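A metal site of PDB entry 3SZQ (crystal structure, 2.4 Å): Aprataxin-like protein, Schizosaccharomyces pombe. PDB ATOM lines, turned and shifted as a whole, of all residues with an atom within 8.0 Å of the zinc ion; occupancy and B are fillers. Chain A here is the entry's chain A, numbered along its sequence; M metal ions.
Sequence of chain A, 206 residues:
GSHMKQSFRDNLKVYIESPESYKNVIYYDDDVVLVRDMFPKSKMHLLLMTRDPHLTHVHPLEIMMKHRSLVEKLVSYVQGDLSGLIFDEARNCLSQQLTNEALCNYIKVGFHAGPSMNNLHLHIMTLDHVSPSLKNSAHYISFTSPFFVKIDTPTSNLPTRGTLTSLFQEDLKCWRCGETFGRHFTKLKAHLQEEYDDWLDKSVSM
The zinc ion is bound by the side-chain carboxylate (OE2) of Glu 195 (2.0 Å), a ring nitrogen (NE2) of His 191 (2.2 Å), the side-chain sulfur (SG) of Cys 174 (2.3 Å) and the side-chain sulfur (SG) of Cys 177 (2.6 Å).
The zinc ion has four donor atoms within binding distance.
Four residues have an atom within 4 Å of the zinc ion: Cys 174, Cys 177, His 191 and Glu 195.
The backbone NH of Cys 174 is in hydrogen-bond range of the backbone carbonyl oxygen of Glu 179 (2.8 Å).
OE1 of Glu 195 lies within salt-bridge range of NH1 of Arg 176 (2.9 Å).
SG of Cys 174 sits close to N of Arg 176 (3.4 Å).
The side-chain sulfur (SG) of Cys 177 lies close to the backbone NH (N) of Glu 179 (3.3 Å).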
ATOM      1  N   TYR A 140      26.690   1.563 -13.182  1.00  0.00           N
ATOM      2  CA  TYR A 140      25.612   2.137 -12.405  1.00  0.00           C
ATOM      3  C   TYR A 140      24.344   1.289 -12.437  1.00  0.00           C
ATOM      4  O   TYR A 140      23.740   1.021 -11.402  1.00  0.00           O
ATOM      5  CB  TYR A 140      25.312   3.562 -12.876  1.00  0.00           C
ATOM      6  CG  TYR A 140      24.148   4.206 -12.153  1.00  0.00           C
ATOM      7  CD1 TYR A 140      24.295   4.733 -10.887  1.00  0.00           C
ATOM      8  CD2 TYR A 140      22.888   4.275 -12.752  1.00  0.00           C
ATOM      9  CE1 TYR A 140      23.228   5.311 -10.217  1.00  0.00           C
ATOM     10  CE2 TYR A 140      21.817   4.856 -12.105  1.00  0.00           C
ATOM     11  CZ  TYR A 140      21.995   5.364 -10.829  1.00  0.00           C
ATOM     12  OH  TYR A 140      20.924   5.945 -10.182  1.00  0.00           O
ATOM     13  N   LYS A 173      18.567   6.649 -14.467  1.00  0.00           N
ATOM     14  CA  LYS A 173      17.645   7.219 -13.491  1.00  0.00           C
ATOM     15  C   LYS A 173      18.305   7.313 -12.108  1.00  0.00           C
ATOM     16  O   LYS A 173      18.875   6.331 -11.625  1.00  0.00           O
ATOM     17  CB  LYS A 173      16.389   6.349 -13.418  1.00  0.00           C
ATOM     18  CG  LYS A 173      15.244   6.925 -12.632  1.00  0.00           C
ATOM     19  CD  LYS A 173      14.100   5.911 -12.578  1.00  0.00           C
ATOM     20  CE  LYS A 173      12.854   6.477 -11.908  1.00  0.00           C
ATOM     21  NZ  LYS A 173      12.409   7.711 -12.609  1.00  0.00           N
ATOM     22  N   CYS A 174      18.251   8.487 -11.487  1.00  0.00           N
ATOM     23  CA  CYS A 174      18.720   8.627 -10.114  1.00  0.00           C
ATOM     24  C   CYS A 174      17.964   7.687  -9.181  1.00  0.00           C
ATOM     25  O   CYS A 174      16.735   7.678  -9.171  1.00  0.00           O
ATOM     26  CB  CYS A 174      18.562  10.057  -9.623  1.00  0.00           C
ATOM     27  SG  CYS A 174      19.157  10.315  -7.945  1.00  0.00           S
ATOM     28  N   TRP A 175      18.702   6.894  -8.408  1.00  0.00           N
ATOM     29  CA  TRP A 175      18.101   5.918  -7.503  1.00  0.00           C
ATOM     30  C   TRP A 175      17.373   6.620  -6.357  1.00  0.00           C
ATOM     31  O   TRP A 175      16.428   6.085  -5.786  1.00  0.00           O
ATOM     32  CB  TRP A 175      19.163   4.958  -6.970  1.00  0.00           C
ATOM     33  CG  TRP A 175      20.191   5.660  -6.139  1.00  0.00           C
ATOM     34  CD1 TRP A 175      21.391   6.161  -6.559  1.00  0.00           C
ATOM     35  CD2 TRP A 175      20.086   5.999  -4.743  1.00  0.00           C
ATOM     36  NE1 TRP A 175      22.039   6.777  -5.524  1.00  0.00           N
ATOM     37  CE2 TRP A 175      21.253   6.692  -4.390  1.00  0.00           C
ATOM     38  CE3 TRP A 175      19.103   5.779  -3.769  1.00  0.00           C
ATOM     39  CZ2 TRP A 175      21.493   7.161  -3.096  1.00  0.00           C
ATOM     40  CZ3 TRP A 175      19.335   6.244  -2.478  1.00  0.00           C
ATOM     41  CH2 TRP A 175      20.519   6.932  -2.157  1.00  0.00           C
ATOM     42  N   ARG A 176      17.811   7.829  -6.017  1.00  0.00           N
ATOM     43  CA  ARG A 176      17.274   8.534  -4.862  1.00  0.00           C
ATOM     44  C   ARG A 176      16.033   9.408  -5.148  1.00  0.00           C
ATOM     45  O   ARG A 176      15.073   9.398  -4.364  1.00  0.00           O
ATOM     46  CB  ARG A 176      18.373   9.387  -4.205  1.00  0.00           C
ATOM     47  CG  ARG A 176      18.002   9.912  -2.827  1.00  0.00           C
ATOM     48  CD  ARG A 176      19.232  10.481  -2.090  1.00  0.00           C
ATOM     49  NE  ARG A 176      18.910  10.906  -0.725  1.00  0.00           N
ATOM     50  CZ  ARG A 176      18.927  12.166  -0.307  1.00  0.00           C
ATOM     51  NH1 ARG A 176      19.259  13.149  -1.144  1.00  0.00           N
ATOM     52  NH2 ARG A 176      18.630  12.452   0.955  1.00  0.00           N
ATOM     53  N   CYS A 177      16.052  10.168  -6.243  1.00  0.00           N
ATOM     54  CA  CYS A 177      14.956  11.097  -6.507  1.00  0.00           C
ATOM     55  C   CYS A 177      14.142  10.807  -7.754  1.00  0.00           C
ATOM     56  O   CYS A 177      13.122  11.453  -7.983  1.00  0.00           O
ATOM     57  CB  CYS A 177      15.478  12.528  -6.584  1.00  0.00           C
ATOM     58  SG  CYS A 177      16.068  12.911  -8.230  1.00  0.00           S
ATOM     59  N   GLY A 178      14.574   9.853  -8.574  1.00  0.00           N
ATOM     60  CA  GLY A 178      13.823   9.488  -9.763  1.00  0.00           C
ATOM     61  C   GLY A 178      14.124  10.273 -11.043  1.00  0.00           C
ATOM     62  O   GLY A 178      13.633   9.903 -12.123  1.00  0.00           O
ATOM     63  N   GLU A 179      14.915  11.337 -10.950  1.00  0.00           N
ATOM     64  CA  GLU A 179      15.265  12.124 -12.129  1.00  0.00           C
ATOM     65  C   GLU A 179      15.955  11.275 -13.204  1.00  0.00           C
ATOM     66  O   GLU A 179      16.732  10.375 -12.895  1.00  0.00           O
ATOM     67  CB  GLU A 179      16.151  13.317 -11.754  1.00  0.00           C
ATOM     68  CG  GLU A 179      16.408  14.261 -12.916  1.00  0.00           C
ATOM     69  CD  GLU A 179      17.204  15.484 -12.514  1.00  0.00           C
ATOM     70  OE1 GLU A 179      17.280  15.779 -11.301  1.00  0.00           O
ATOM     71  OE2 GLU A 179      17.760  16.151 -13.412  1.00  0.00           O
ATOM     72  N   THR A 180      15.663  11.596 -14.464  1.00  0.00           N
ATOM     73  CA  THR A 180      16.196  10.850 -15.615  1.00  0.00           C
ATOM     74  C   THR A 180      17.281  11.633 -16.358  1.00  0.00           C
ATOM     75  O   THR A 180      17.289  12.872 -16.343  1.00  0.00           O
ATOM     76  CB  THR A 180      15.066  10.487 -16.595  1.00  0.00           C
ATOM     77  OG1 THR A 180      14.364  11.674 -16.981  1.00  0.00           O
ATOM     78  CG2 THR A 180      14.086   9.515 -15.938  1.00  0.00           C
ATOM     79  N   PHE A 181      18.207  10.924 -16.994  1.00  0.00           N
ATOM     80  CA  PHE A 181      19.345  11.584 -17.624  1.00  0.00           C
ATOM     81  C   PHE A 181      19.663  11.024 -19.006  1.00  0.00           C
ATOM     82  O   PHE A 181      20.729  11.273 -19.558  1.00  0.00           O
ATOM     83  CB  PHE A 181      20.580  11.505 -16.721  1.00  0.00           C
ATOM     84  CG  PHE A 181      20.433  12.263 -15.436  1.00  0.00           C
ATOM     85  CD1 PHE A 181      20.797  13.593 -15.370  1.00  0.00           C
ATOM     86  CD2 PHE A 181      19.912  11.648 -14.305  1.00  0.00           C
ATOM     87  CE1 PHE A 181      20.647  14.304 -14.185  1.00  0.00           C
ATOM     88  CE2 PHE A 181      19.770  12.356 -13.131  1.00  0.00           C
ATOM     89  CZ  PHE A 181      20.134  13.685 -13.065  1.00  0.00           C
ATOM     90  N   LEU A 188      24.592  12.305 -14.832  1.00  0.00           N
ATOM     91  CA  LEU A 188      24.255  11.472 -13.682  1.00  0.00           C
ATOM     92  C   LEU A 188      25.349  11.595 -12.606  1.00  0.00           C
ATOM     93  O   LEU A 188      25.050  11.863 -11.453  1.00  0.00           O
ATOM     94  CB  LEU A 188      24.069  10.014 -14.114  1.00  0.00           C
ATOM     95  CG  LEU A 188      23.759   9.023 -12.997  1.00  0.00           C
ATOM     96  CD1 LEU A 188      22.349   9.219 -12.463  1.00  0.00           C
ATOM     97  CD2 LEU A 188      23.939   7.594 -13.483  1.00  0.00           C
ATOM     98  N   HIS A 191      25.192  14.663 -10.724  1.00  0.00           N
ATOM     99  CA  HIS A 191      23.993  14.621  -9.916  1.00  0.00           C
ATOM    100  C   HIS A 191      24.168  13.726  -8.684  1.00  0.00           C
ATOM    101  O   HIS A 191      23.754  14.096  -7.588  1.00  0.00           O
ATOM    102  CB  HIS A 191      22.790  14.174 -10.748  1.00  0.00           C
ATOM    103  CG  HIS A 191      21.502  14.222  -9.987  1.00  0.00           C
ATOM    104  ND1 HIS A 191      20.864  15.403  -9.679  1.00  0.00           N
ATOM    105  CD2 HIS A 191      20.744  13.232  -9.469  1.00  0.00           C
ATOM    106  CE1 HIS A 191      19.763  15.146  -9.015  1.00  0.00           C
ATOM    107  NE2 HIS A 191      19.662  13.832  -8.871  1.00  0.00           N
ATOM    108  N   LEU A 192      24.788  12.554  -8.857  1.00  0.00           N
ATOM    109  CA  LEU A 192      25.033  11.666  -7.730  1.00  0.00           C
ATOM    110  C   LEU A 192      25.828  12.382  -6.652  1.00  0.00           C
ATOM    111  O   LEU A 192      25.556  12.235  -5.468  1.00  0.00           O
ATOM    112  CB  LEU A 192      25.754  10.383  -8.178  1.00  0.00           C
ATOM    113  CG  LEU A 192      24.893   9.508  -9.086  1.00  0.00           C
ATOM    114  CD1 LEU A 192      25.690   8.446  -9.797  1.00  0.00           C
ATOM    115  CD2 LEU A 192      23.761   8.875  -8.285  1.00  0.00           C
ATOM    116  N   GLU A 194      25.826  15.528  -5.942  1.00  0.00           N
ATOM    117  CA  GLU A 194      24.919  16.462  -5.267  1.00  0.00           C
ATOM    118  C   GLU A 194      23.980  15.720  -4.330  1.00  0.00           C
ATOM    119  O   GLU A 194      23.686  16.184  -3.232  1.00  0.00           O
ATOM    120  CB  GLU A 194      24.077  17.236  -6.296  1.00  0.00           C
ATOM    121  CG  GLU A 194      24.842  18.111  -7.278  1.00  0.00           C
ATOM    122  CD  GLU A 194      23.979  18.547  -8.476  1.00  0.00           C
ATOM    123  OE1 GLU A 194      22.798  18.910  -8.264  1.00  0.00           O
ATOM    124  OE2 GLU A 194      24.477  18.511  -9.615  1.00  0.00           O
ATOM    125  N   GLU A 195      23.487  14.569  -4.779  1.00  0.00           N
ATOM    126  CA  GLU A 195      22.609  13.733  -3.971  1.00  0.00           C
ATOM    127  C   GLU A 195      23.329  13.305  -2.712  1.00  0.00           C
ATOM    128  O   GLU A 195      22.718  13.221  -1.639  1.00  0.00           O
ATOM    129  CB  GLU A 195      22.162  12.490  -4.754  1.00  0.00           C
ATOM    130  CG  GLU A 195      21.051  12.731  -5.746  1.00  0.00           C
ATOM    131  CD  GLU A 195      19.758  13.194  -5.089  1.00  0.00           C
ATOM    132  OE1 GLU A 195      19.785  13.646  -3.927  1.00  0.00           O
ATOM    133  OE2 GLU A 195      18.702  13.123  -5.752  1.00  0.00           O
ATOM    134  N   TYR A 196      24.621  13.012  -2.822  1.00  0.00           N
ATOM    135  CA  TYR A 196      25.380  12.555  -1.668  1.00  0.00           C
ATOM    136  C   TYR A 196      25.593  13.682  -0.664  1.00  0.00           C
ATOM    137  O   TYR A 196      25.397  13.493   0.540  1.00  0.00           O
ATOM    138  CB  TYR A 196      26.722  11.922  -2.068  1.00  0.00           C
ATOM    139  CG  TYR A 196      27.611  11.666  -0.873  1.00  0.00           C
ATOM    140  CD1 TYR A 196      27.366  10.601  -0.021  1.00  0.00           C
ATOM    141  CD2 TYR A 196      28.690  12.498  -0.599  1.00  0.00           C
ATOM    142  CE1 TYR A 196      28.161  10.365   1.062  1.00  0.00           C
ATOM    143  CE2 TYR A 196      29.499  12.267   0.501  1.00  0.00           C
ATOM    144  CZ  TYR A 196      29.234  11.196   1.324  1.00  0.00           C
ATOM    145  OH  TYR A 196      30.030  10.944   2.422  1.00  0.00           O
HETATM  146 ZN    ZN M   1      18.515  12.460  -7.648  1.00  0.00          ZN
